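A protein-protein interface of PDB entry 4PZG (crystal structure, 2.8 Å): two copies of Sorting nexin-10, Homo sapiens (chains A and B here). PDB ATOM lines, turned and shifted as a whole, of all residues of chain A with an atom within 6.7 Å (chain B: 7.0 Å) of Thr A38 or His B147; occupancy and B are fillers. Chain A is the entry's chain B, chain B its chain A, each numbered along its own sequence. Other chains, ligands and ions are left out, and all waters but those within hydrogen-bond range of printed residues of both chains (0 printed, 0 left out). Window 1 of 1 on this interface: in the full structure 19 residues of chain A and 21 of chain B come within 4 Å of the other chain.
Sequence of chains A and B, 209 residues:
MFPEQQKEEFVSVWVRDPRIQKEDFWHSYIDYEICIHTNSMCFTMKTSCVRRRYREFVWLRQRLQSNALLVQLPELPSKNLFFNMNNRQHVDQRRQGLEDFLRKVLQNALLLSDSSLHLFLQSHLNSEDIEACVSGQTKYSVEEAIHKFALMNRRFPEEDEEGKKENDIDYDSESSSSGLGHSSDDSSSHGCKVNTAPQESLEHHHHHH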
ATOM      1  N   GLU A   9     -35.760 -30.117  10.870  1.00  0.00           N
ATOM      2  CA  GLU A   9     -35.289 -28.786  11.254  1.00  0.00           C
ATOM      3  C   GLU A   9     -34.755 -28.717  12.717  1.00  0.00           C
ATOM      4  O   GLU A   9     -35.381 -29.223  13.642  1.00  0.00           O
ATOM      5  CB  GLU A   9     -36.404 -27.732  11.022  1.00  0.00           C
ATOM      6  CG  GLU A   9     -36.861 -27.569   9.560  1.00  0.00           C
ATOM      7  CD  GLU A   9     -37.265 -26.122   9.163  1.00  0.00           C
ATOM      8  OE1 GLU A   9     -37.110 -25.732   7.968  1.00  0.00           O
ATOM      9  OE2 GLU A   9     -37.727 -25.349  10.036  1.00  0.00           O
ATOM     10  N   PHE A  10     -33.587 -28.107  12.914  1.00  0.00           N
ATOM     11  CA  PHE A  10     -33.101 -27.818  14.255  1.00  0.00           C
ATOM     12  C   PHE A  10     -32.534 -26.427  14.285  1.00  0.00           C
ATOM     13  O   PHE A  10     -32.141 -25.879  13.250  1.00  0.00           O
ATOM     14  CB  PHE A  10     -32.057 -28.831  14.717  1.00  0.00           C
ATOM     15  CG  PHE A  10     -30.749 -28.707  14.014  1.00  0.00           C
ATOM     16  CD1 PHE A  10     -30.583 -29.245  12.741  1.00  0.00           C
ATOM     17  CD2 PHE A  10     -29.693 -28.038  14.604  1.00  0.00           C
ATOM     18  CE1 PHE A  10     -29.387 -29.110  12.055  1.00  0.00           C
ATOM     19  CE2 PHE A  10     -28.474 -27.897  13.929  1.00  0.00           C
ATOM     20  CZ  PHE A  10     -28.332 -28.424  12.647  1.00  0.00           C
ATOM     21  N   VAL A  11     -32.505 -25.850  15.476  1.00  0.00           N
ATOM     22  CA  VAL A  11     -31.784 -24.587  15.700  1.00  0.00           C
ATOM     23  C   VAL A  11     -31.025 -24.630  17.010  1.00  0.00           C
ATOM     24  O   VAL A  11     -31.558 -25.037  18.010  1.00  0.00           O
ATOM     25  CB  VAL A  11     -32.746 -23.396  15.636  1.00  0.00           C
ATOM     26  CG1 VAL A  11     -33.967 -23.682  16.459  1.00  0.00           C
ATOM     27  CG2 VAL A  11     -32.064 -22.137  16.132  1.00  0.00           C
ATOM     28  N   SER A  12     -29.769 -24.262  17.008  1.00  0.00           N
ATOM     29  CA  SER A  12     -28.972 -24.330  18.228  1.00  0.00           C
ATOM     30  C   SER A  12     -28.245 -23.041  18.425  1.00  0.00           C
ATOM     31  O   SER A  12     -27.731 -22.446  17.480  1.00  0.00           O
ATOM     32  CB  SER A  12     -27.936 -25.432  18.139  1.00  0.00           C
ATOM     33  OG  SER A  12     -28.596 -26.637  17.843  1.00  0.00           O
ATOM     34  N   ILE A  36     -24.934 -19.352  16.271  1.00  0.00           N
ATOM     35  CA  ILE A  36     -26.112 -20.064  15.837  1.00  0.00           C
ATOM     36  C   ILE A  36     -25.676 -21.188  14.917  1.00  0.00           C
ATOM     37  O   ILE A  36     -24.788 -21.002  14.061  1.00  0.00           O
ATOM     38  CB  ILE A  36     -26.994 -19.124  15.016  1.00  0.00           C
ATOM     39  CG1 ILE A  36     -27.595 -18.060  15.910  1.00  0.00           C
ATOM     40  CG2 ILE A  36     -28.085 -19.869  14.260  1.00  0.00           C
ATOM     41  CD1 ILE A  36     -28.613 -18.596  16.873  1.00  0.00           C
ATOM     42  N   HIS A  37     -26.309 -22.347  15.050  1.00  0.00           N
ATOM     43  CA  HIS A  37     -26.192 -23.389  14.014  1.00  0.00           C
ATOM     44  C   HIS A  37     -27.536 -23.947  13.741  1.00  0.00           C
ATOM     45  O   HIS A  37     -28.228 -24.378  14.644  1.00  0.00           O
ATOM     46  CB  HIS A  37     -25.284 -24.503  14.428  1.00  0.00           C
ATOM     47  CG  HIS A  37     -25.103 -25.545  13.372  1.00  0.00           C
ATOM     48  ND1 HIS A  37     -24.981 -26.883  13.664  1.00  0.00           N
ATOM     49  CD2 HIS A  37     -25.064 -25.450  12.025  1.00  0.00           C
ATOM     50  CE1 HIS A  37     -24.842 -27.561  12.542  1.00  0.00           C
ATOM     51  NE2 HIS A  37     -24.888 -26.716  11.535  1.00  0.00           N
ATOM     52  N   THR A  38     -27.969 -23.873  12.503  1.00  0.00           N
ATOM     53  CA  THR A  38     -29.313 -24.345  12.206  1.00  0.00           C
ATOM     54  C   THR A  38     -29.314 -24.926  10.810  1.00  0.00           C
ATOM     55  O   THR A  38     -28.481 -24.557   9.973  1.00  0.00           O
ATOM     56  CB  THR A  38     -30.343 -23.196  12.261  1.00  0.00           C
ATOM     57  OG1 THR A  38     -31.649 -23.717  12.021  1.00  0.00           O
ATOM     58  CG2 THR A  38     -30.043 -22.134  11.202  1.00  0.00           C
ATOM     59  N   ASN A  39     -30.296 -25.752  10.549  1.00  0.00           N
ATOM     60  CA  ASN A  39     -30.619 -26.062   9.189  1.00  0.00           C
ATOM     61  C   ASN A  39     -32.014 -25.535   8.761  1.00  0.00           C
ATOM     62  O   ASN A  39     -32.603 -26.035   7.827  1.00  0.00           O
ATOM     63  CB  ASN A  39     -30.591 -27.554   9.042  1.00  0.00           C
ATOM     64  CG  ASN A  39     -31.728 -28.173   9.743  1.00  0.00           C
ATOM     65  OD1 ASN A  39     -32.698 -27.479  10.068  1.00  0.00           O
ATOM     66  ND2 ASN A  39     -31.652 -29.459   9.976  1.00  0.00           N
ATOM     67  N   SER A  40     -32.531 -24.524   9.429  1.00  0.00           N
ATOM     68  CA  SER A  40     -33.884 -24.093   9.187  1.00  0.00           C
ATOM     69  C   SER A  40     -33.948 -23.060   8.085  1.00  0.00           C
ATOM     70  O   SER A  40     -33.024 -22.316   7.867  1.00  0.00           O
ATOM     71  CB  SER A  40     -34.446 -23.532  10.487  1.00  0.00           C
ATOM     72  OG  SER A  40     -35.503 -22.610  10.273  1.00  0.00           O
ATOM     73  N   MET A  41     -35.079 -23.002   7.405  1.00  0.00           N
ATOM     74  CA  MET A  41     -35.328 -22.000   6.365  1.00  0.00           C
ATOM     75  C   MET A  41     -35.617 -20.640   6.987  1.00  0.00           C
ATOM     76  O   MET A  41     -35.567 -19.617   6.307  1.00  0.00           O
ATOM     77  CB  MET A  41     -36.520 -22.451   5.497  1.00  0.00           C
ATOM     78  CG  MET A  41     -36.370 -23.812   4.785  1.00  0.00           C
ATOM     79  SD  MET A  41     -35.039 -23.909   3.541  1.00  0.00           S
ATOM     80  CE  MET A  41     -33.633 -24.711   4.376  1.00  0.00           C
ATOM     81  N   CYS A  42     -35.887 -20.627   8.292  1.00  0.00           N
ATOM     82  CA  CYS A  42     -36.161 -19.385   9.015  1.00  0.00           C
ATOM     83  C   CYS A  42     -34.987 -18.416   9.027  1.00  0.00           C
ATOM     84  O   CYS A  42     -35.182 -17.219   8.847  1.00  0.00           O
ATOM     85  CB  CYS A  42     -36.642 -19.670  10.434  1.00  0.00           C
ATOM     86  SG  CYS A  42     -38.307 -20.441  10.343  1.00  0.00           S
ATOM     87  N   PHE A  43     -33.778 -18.954   9.158  1.00  0.00           N
ATOM     88  CA  PHE A  43     -32.574 -18.164   9.164  1.00  0.00           C
ATOM     89  C   PHE A  43     -31.989 -18.002   7.805  1.00  0.00           C
ATOM     90  O   PHE A  43     -32.117 -18.890   6.998  1.00  0.00           O
ATOM     91  CB  PHE A  43     -31.543 -18.803  10.075  1.00  0.00           C
ATOM     92  CG  PHE A  43     -31.904 -18.682  11.500  1.00  0.00           C
ATOM     93  CD1 PHE A  43     -32.891 -19.499  12.035  1.00  0.00           C
ATOM     94  CD2 PHE A  43     -31.358 -17.663  12.277  1.00  0.00           C
ATOM     95  CE1 PHE A  43     -33.268 -19.346  13.346  1.00  0.00           C
ATOM     96  CE2 PHE A  43     -31.740 -17.498  13.590  1.00  0.00           C
ATOM     97  CZ  PHE A  43     -32.690 -18.334  14.121  1.00  0.00           C
ATOM     98  N   THR A  44     -31.337 -16.869   7.565  1.00  0.00           N
ATOM     99  CA  THR A  44     -30.641 -16.626   6.339  1.00  0.00           C
ATOM    100  C   THR A  44     -29.376 -17.477   6.246  1.00  0.00           C
ATOM    101  O   THR A  44     -29.164 -18.192   5.293  1.00  0.00           O
ATOM    102  CB  THR A  44     -30.280 -15.136   6.216  1.00  0.00           C
ATOM    103  OG1 THR A  44     -31.460 -14.383   6.018  1.00  0.00           O
ATOM    104  CG2 THR A  44     -29.424 -14.881   5.017  1.00  0.00           C
ATOM    105  N   MET A  45     -28.520 -17.366   7.236  1.00  0.00           N
ATOM    106  CA  MET A  45     -27.283 -18.096   7.283  1.00  0.00           C
ATOM    107  C   MET A  45     -27.452 -19.299   8.179  1.00  0.00           C
ATOM    108  O   MET A  45     -28.147 -19.216   9.171  1.00  0.00           O
ATOM    109  CB  MET A  45     -26.237 -17.201   7.899  1.00  0.00           C
ATOM    110  CG  MET A  45     -25.939 -16.007   7.041  1.00  0.00           C
ATOM    111  SD  MET A  45     -25.170 -16.562   5.530  1.00  0.00           S
ATOM    112  CE  MET A  45     -25.301 -15.136   4.453  1.00  0.00           C
ATOM    113  N   LYS A  46     -26.787 -20.400   7.864  1.00  0.00           N
ATOM    114  CA  LYS A  46     -26.952 -21.622   8.636  1.00  0.00           C
ATOM    115  C   LYS A  46     -25.986 -21.646   9.791  1.00  0.00           C
ATOM    116  O   LYS A  46     -26.181 -22.413  10.735  1.00  0.00           O
ATOM    117  CB  LYS A  46     -26.688 -22.836   7.773  1.00  0.00           C
ATOM    118  CG  LYS A  46     -27.509 -22.919   6.521  1.00  0.00           C
ATOM    119  CD  LYS A  46     -28.982 -22.940   6.819  1.00  0.00           C
ATOM    120  CE  LYS A  46     -29.775 -22.938   5.534  1.00  0.00           C
ATOM    121  NZ  LYS A  46     -31.124 -22.345   5.778  1.00  0.00           N
ATOM    122  N   THR A  47     -24.945 -20.830   9.715  1.00  0.00           N
ATOM    123  CA  THR A  47     -24.143 -20.593  10.881  1.00  0.00           C
ATOM    124  C   THR A  47     -23.884 -19.143  11.009  1.00  0.00           C
ATOM    125  O   THR A  47     -23.872 -18.438  10.022  1.00  0.00           O
ATOM    126  CB  THR A  47     -22.761 -21.254  10.839  1.00  0.00           C
ATOM    127  OG1 THR A  47     -21.890 -20.533   9.962  1.00  0.00           O
ATOM    128  CG2 THR A  47     -22.869 -22.690  10.476  1.00  0.00           C
ATOM    129  N   GLN A 122     -27.301 -12.165  13.307  1.00  0.00           N
ATOM    130  CA  GLN A 122     -26.564 -12.453  12.122  1.00  0.00           C
ATOM    131  C   GLN A 122     -26.027 -11.240  11.420  1.00  0.00           C
ATOM    132  O   GLN A 122     -25.780 -11.312  10.237  1.00  0.00           O
ATOM    133  CB  GLN A 122     -27.434 -13.291  11.194  1.00  0.00           C
ATOM    134  CG  GLN A 122     -27.853 -14.567  11.887  1.00  0.00           C
ATOM    135  CD  GLN A 122     -28.185 -15.734  10.961  1.00  0.00           C
ATOM    136  OE1 GLN A 122     -28.981 -15.626  10.026  1.00  0.00           O
ATOM    137  NE2 GLN A 122     -27.638 -16.889  11.285  1.00  0.00           N
ATOM    138  N   THR B  44     -27.377 -25.213   0.030  1.00  0.00           N
ATOM    139  CA  THR B  44     -27.446 -25.324   1.477  1.00  0.00           C
ATOM    140  C   THR B  44     -26.801 -24.104   2.188  1.00  0.00           C
ATOM    141  O   THR B  44     -27.447 -23.456   2.993  1.00  0.00           O
ATOM    142  CB  THR B  44     -26.752 -26.580   1.937  1.00  0.00           C
ATOM    143  OG1 THR B  44     -27.496 -27.709   1.505  1.00  0.00           O
ATOM    144  CG2 THR B  44     -26.706 -26.638   3.405  1.00  0.00           C
ATOM    145  N   MET B  45     -25.570 -23.777   1.841  1.00  0.00           N
ATOM    146  CA  MET B  45     -24.864 -22.668   2.418  1.00  0.00           C
ATOM    147  C   MET B  45     -24.870 -21.513   1.459  1.00  0.00           C
ATOM    148  O   MET B  45     -24.717 -21.711   0.291  1.00  0.00           O
ATOM    149  CB  MET B  45     -23.397 -23.059   2.686  1.00  0.00           C
ATOM    150  CG  MET B  45     -23.264 -24.180   3.686  1.00  0.00           C
ATOM    151  SD  MET B  45     -23.819 -23.641   5.301  1.00  0.00           S
ATOM    152  CE  MET B  45     -24.027 -25.170   6.196  1.00  0.00           C
ATOM    153  N   GLN B 122     -19.313 -27.378  -1.781  1.00  0.00           N
ATOM    154  CA  GLN B 122     -19.590 -27.061  -0.405  1.00  0.00           C
ATOM    155  C   GLN B 122     -19.256 -28.205   0.506  1.00  0.00           C
ATOM    156  O   GLN B 122     -19.924 -28.402   1.498  1.00  0.00           O
ATOM    157  CB  GLN B 122     -21.070 -26.683  -0.276  1.00  0.00           C
ATOM    158  CG  GLN B 122     -21.411 -25.509  -1.192  1.00  0.00           C
ATOM    159  CD  GLN B 122     -22.611 -24.665  -0.797  1.00  0.00           C
ATOM    160  OE1 GLN B 122     -23.711 -25.168  -0.482  1.00  0.00           O
ATOM    161  NE2 GLN B 122     -22.421 -23.356  -0.885  1.00  0.00           N
ATOM    162  N   SER B 123     -18.217 -28.958   0.168  1.00  0.00           N
ATOM    163  CA  SER B 123     -17.659 -29.938   1.062  1.00  0.00           C
ATOM    164  C   SER B 123     -16.240 -30.289   0.759  1.00  0.00           C
ATOM    165  O   SER B 123     -15.738 -30.085  -0.326  1.00  0.00           O
ATOM    166  CB  SER B 123     -18.496 -31.225   1.087  1.00  0.00           C
ATOM    167  OG  SER B 123     -18.271 -32.061  -0.035  1.00  0.00           O
ATOM    168  N   VAL B 142     -25.986 -35.948   2.434  1.00  0.00           N
ATOM    169  CA  VAL B 142     -25.387 -34.850   1.706  1.00  0.00           C
ATOM    170  C   VAL B 142     -25.432 -33.599   2.580  1.00  0.00           C
ATOM    171  O   VAL B 142     -24.437 -32.883   2.674  1.00  0.00           O
ATOM    172  CB  VAL B 142     -26.151 -34.616   0.365  1.00  0.00           C
ATOM    173  CG1 VAL B 142     -25.711 -33.355  -0.324  1.00  0.00           C
ATOM    174  CG2 VAL B 142     -25.942 -35.773  -0.579  1.00  0.00           C
ATOM    175  N   GLU B 143     -26.582 -33.354   3.222  1.00  0.00           N
ATOM    176  CA  GLU B 143     -26.738 -32.168   4.068  1.00  0.00           C
ATOM    177  C   GLU B 143     -25.774 -32.301   5.214  1.00  0.00           C
ATOM    178  O   GLU B 143     -25.034 -31.392   5.502  1.00  0.00           O
ATOM    179  CB  GLU B 143     -28.156 -31.979   4.571  1.00  0.00           C
ATOM    180  CG  GLU B 143     -29.264 -32.305   3.547  1.00  0.00           C
ATOM    181  CD  GLU B 143     -29.466 -31.256   2.442  1.00  0.00           C
ATOM    182  OE1 GLU B 143     -28.973 -30.105   2.539  1.00  0.00           O
ATOM    183  OE2 GLU B 143     -30.125 -31.607   1.432  1.00  0.00           O
ATOM    184  N   GLU B 144     -25.680 -33.482   5.803  1.00  0.00           N
ATOM    185  CA  GLU B 144     -24.727 -33.651   6.887  1.00  0.00           C
ATOM    186  C   GLU B 144     -23.302 -33.316   6.499  1.00  0.00           C
ATOM    187  O   GLU B 144     -22.587 -32.668   7.235  1.00  0.00           O
ATOM    188  CB  GLU B 144     -24.814 -35.034   7.485  1.00  0.00           C
ATOM    189  CG  GLU B 144     -26.025 -35.146   8.416  1.00  0.00           C
ATOM    190  CD  GLU B 144     -26.497 -36.567   8.650  1.00  0.00           C
ATOM    191  OE1 GLU B 144     -27.733 -36.776   8.742  1.00  0.00           O
ATOM    192  OE2 GLU B 144     -25.647 -37.481   8.719  1.00  0.00           O
ATOM    193  N   ALA B 145     -22.898 -33.684   5.306  1.00  0.00           N
ATOM    194  CA  ALA B 145     -21.518 -33.487   4.932  1.00  0.00           C
ATOM    195  C   ALA B 145     -21.214 -32.031   4.756  1.00  0.00           C
ATOM    196  O   ALA B 145     -20.121 -31.583   5.007  1.00  0.00           O
ATOM    197  CB  ALA B 145     -21.256 -34.205   3.635  1.00  0.00           C
ATOM    198  N   ILE B 146     -22.202 -31.315   4.231  1.00  0.00           N
ATOM    199  CA  ILE B 146     -22.060 -29.901   3.919  1.00  0.00           C
ATOM    200  C   ILE B 146     -21.995 -29.061   5.188  1.00  0.00           C
ATOM    201  O   ILE B 146     -21.139 -28.162   5.291  1.00  0.00           O
ATOM    202  CB  ILE B 146     -23.218 -29.412   3.019  1.00  0.00           C
ATOM    203  CG1 ILE B 146     -23.070 -30.016   1.628  1.00  0.00           C
ATOM    204  CG2 ILE B 146     -23.164 -27.914   2.863  1.00  0.00           C
ATOM    205  CD1 ILE B 146     -24.186 -29.711   0.652  1.00  0.00           C
ATOM    206  N   HIS B 147     -22.899 -29.372   6.126  1.00  0.00           N
ATOM    207  CA  HIS B 147     -22.886 -28.752   7.432  1.00  0.00           C
ATOM    208  C   HIS B 147     -21.584 -29.061   8.147  1.00  0.00           C
ATOM    209  O   HIS B 147     -20.925 -28.162   8.617  1.00  0.00           O
ATOM    210  CB  HIS B 147     -24.077 -29.183   8.253  1.00  0.00           C
ATOM    211  CG  HIS B 147     -25.342 -28.491   7.874  1.00  0.00           C
ATOM    212  ND1 HIS B 147     -25.795 -27.356   8.507  1.00  0.00           N
ATOM    213  CD2 HIS B 147     -26.250 -28.762   6.909  1.00  0.00           C
ATOM    214  CE1 HIS B 147     -26.932 -26.969   7.958  1.00  0.00           C
ATOM    215  NE2 HIS B 147     -27.231 -27.802   6.984  1.00  0.00           N
ATOM    216  N   LYS B 148     -21.149 -30.310   8.166  1.00  0.00           N
ATOM    217  CA  LYS B 148     -19.897 -30.618   8.828  1.00  0.00           C
ATOM    218  C   LYS B 148     -18.727 -29.876   8.213  1.00  0.00           C
ATOM    219  O   LYS B 148     -17.795 -29.498   8.886  1.00  0.00           O
ATOM    220  CB  LYS B 148     -19.641 -32.117   8.816  1.00  0.00           C
ATOM    221  CG  LYS B 148     -18.288 -32.520   9.399  1.00  0.00           C
ATOM    222  CD  LYS B 148     -18.051 -34.044   9.473  1.00  0.00           C
ATOM    223  CE  LYS B 148     -16.618 -34.394   9.983  1.00  0.00           C
ATOM    224  NZ  LYS B 148     -15.776 -35.192   9.014  1.00  0.00           N
ATOM    225  N   PHE B 149     -18.774 -29.616   6.929  1.00  0.00           N
ATOM    226  CA  PHE B 149     -17.697 -28.864   6.301  1.00  0.00           C
ATOM    227  C   PHE B 149     -17.695 -27.412   6.753  1.00  0.00           C
ATOM    228  O   PHE B 149     -16.644 -26.863   7.040  1.00  0.00           O
ATOM    229  CB  PHE B 149     -17.854 -28.857   4.806  1.00  0.00           C
ATOM    230  CG  PHE B 149     -16.821 -28.052   4.118  1.00  0.00           C
ATOM    231  CD1 PHE B 149     -15.452 -28.362   4.313  1.00  0.00           C
ATOM    232  CD2 PHE B 149     -17.182 -26.998   3.283  1.00  0.00           C
ATOM    233  CE1 PHE B 149     -14.450 -27.622   3.680  1.00  0.00           C
ATOM    234  CE2 PHE B 149     -16.204 -26.264   2.629  1.00  0.00           C
ATOM    235  CZ  PHE B 149     -14.844 -26.561   2.833  1.00  0.00           C
ATOM    236  N   ALA B 150     -18.876 -26.795   6.790  1.00  0.00           N
ATOM    237  CA  ALA B 150     -18.985 -25.421   7.205  1.00  0.00           C
ATOM    238  C   ALA B 150     -18.514 -25.282   8.660  1.00  0.00           C
ATOM    239  O   ALA B 150     -17.673 -24.421   8.950  1.00  0.00           O
ATOM    240  CB  ALA B 150     -20.407 -24.937   7.035  1.00  0.00           C
ATOM    241  N   LEU B 151     -18.991 -26.161   9.558  1.00  0.00           N
ATOM    242  CA  LEU B 151     -18.511 -26.126  10.943  1.00  0.00           C
ATOM    243  C   LEU B 151     -16.976 -26.254  11.005  1.00  0.00           C
ATOM    244  O   LEU B 151     -16.338 -25.398  11.582  1.00  0.00           O
ATOM    245  CB  LEU B 151     -19.162 -27.166  11.806  1.00  0.00           C
ATOM    246  CG  LEU B 151     -20.686 -27.202  11.771  1.00  0.00           C
ATOM    247  CD1 LEU B 151     -21.211 -28.449  12.423  1.00  0.00           C
ATOM    248  CD2 LEU B 151     -21.328 -26.035  12.472  1.00  0.00           C
ATOM    249  N   MET B 152     -16.381 -27.260  10.367  1.00  0.00           N
ATOM    250  CA  MET B 152     -14.917 -27.390  10.391  1.00  0.00           C
ATOM    251  C   MET B 152     -14.290 -26.158   9.813  1.00  0.00           C
ATOM    252  O   MET B 152     -13.298 -25.635  10.309  1.00  0.00           O
ATOM    253  CB  MET B 152     -14.386 -28.566   9.561  1.00  0.00           C
ATOM    254  CG  MET B 152     -14.449 -29.970  10.160  1.00  0.00           C
ATOM    255  SD  MET B 152     -14.351 -31.289   8.872  1.00  0.00           S
ATOM    256  CE  MET B 152     -12.967 -30.771   7.819  1.00  0.00           C
ATOM    257  N   ASN B 153     -14.854 -25.692   8.734  1.00  0.00           N
ATOM    258  CA  ASN B 153     -14.184 -24.683   7.935  1.00  0.00           C
ATOM    259  C   ASN B 153     -14.254 -23.294   8.533  1.00  0.00           C
ATOM    260  O   ASN B 153     -13.405 -22.501   8.306  1.00  0.00           O
ATOM    261  CB  ASN B 153     -14.800 -24.693   6.553  1.00  0.00           C
ATOM    262  CG  ASN B 153     -13.857 -24.249   5.495  1.00  0.00           C
ATOM    263  OD1 ASN B 153     -12.683 -24.557   5.531  1.00  0.00           O
ATOM    264  ND2 ASN B 153     -14.384 -23.554   4.520  1.00  0.00           N
ATOM    265  N   PHE B 156     -16.003 -23.378  13.898  1.00  0.00           N
ATOM    266  CA  PHE B 156     -17.096 -23.143  14.773  1.00  0.00           C
ATOM    267  C   PHE B 156     -16.951 -23.928  16.048  1.00  0.00           C
ATOM    268  O   PHE B 156     -16.722 -25.119  15.999  1.00  0.00           O
ATOM    269  CB  PHE B 156     -18.324 -23.637  14.038  1.00  0.00           C
ATOM    270  CG  PHE B 156     -19.619 -23.187  14.611  1.00  0.00           C
ATOM    271  CD1 PHE B 156     -20.208 -22.010  14.177  1.00  0.00           C
ATOM    272  CD2 PHE B 156     -20.271 -23.977  15.520  1.00  0.00           C
ATOM    273  CE1 PHE B 156     -21.436 -21.615  14.647  1.00  0.00           C
ATOM    274  CE2 PHE B 156     -21.500 -23.595  16.014  1.00  0.00           C
ATOM    275  CZ  PHE B 156     -22.093 -22.411  15.557  1.00  0.00           C
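ND1 of His B147 lies within hydrogen-bond range of NE2 of His A37, at 3.2 Å.
Thr A38 touches just one residue of chain B: His B147. Of chain A, only His A37, Thr A38 and Asn A39 come within 4 Å of His B147. Printed residues of chain A within 4 Å of Thr B44: Lys A46 (3.5 Å). Printed residues of chain A within 4 Å of Leu B151: His A37. Of the printed residues of chain B, His A37 touches His B147 (3.2 Å), Leu B151 (3.7 Å) and Phe B156 (3.98 Å). Printed residues of chain B within 4 Å of Asn A39: His B147 (3.9 Å). Of the printed residues of chain A, Phe B156 touches Ile A36 and His A37. Met A45 touches none of the printed residues of chain B. The nearest residue of chain B that does not touch Thr A38 is Met B45 (5.9 Å). The nearest residue of chain A that does not touch His B147 is Lys A46 (4.1 Å).
Printed residues of chain A that touch a printed residue of chain B: Ile A36, His A37, Thr A38, Asn A39 and Lys A46. Of the 17 printed residues of chain B, 5 touch a printed residue of chain A. Hydrophobic or aromatic side chains of chain B that line the printed part of chain A: Met B45, His B147, Leu B151 and Phe B156. Along chain B the printed residues that touch a printed residue of chain A span positions 44 to 156. Among the printed residues, 8 pairs touch across the chains.
The backbone carbonyl oxygen (O) of Ser A12 sits at hydrogen-bond distance from the backbone NH (N) of His A37 (2.8 Å). O of Leu B151 sits at hydrogen-bond distance from N of Phe B156, at 3.1 Å. The side-chain hydroxyl of Thr A38 lies within hydrogen-bond range of the backbone NH of Ser A40 (2.9 Å). The backbone carbonyl oxygen (O) of Phe A10 sits at hydrogen-bond distance from the side-chain hydroxyl (OG1) of Thr A38. The backbone carbonyl oxygen (O) of Met B45 lies within hydrogen-bond range of the side-chain amide nitrogen (NE2) of Gln B122, 3.1 Å away. The backbone carbonyl oxygen of Lys A46 is in hydrogen-bond range of the backbone NH of Thr A38.
3 positions are printed for both chains. Of the 8 pairs that touch across the chains among the printed residues, none has its exchanged pair printed and touching as well.
Among the printed residues, merely in contact across the chains: Ile A36 with Phe B156, Lys A46 with Thr B44, Thr A38 with His B147, His A37 with Leu B151, Asn A39 with His B147, Lys A46 with Met B45 and His A37 with Phe B156.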
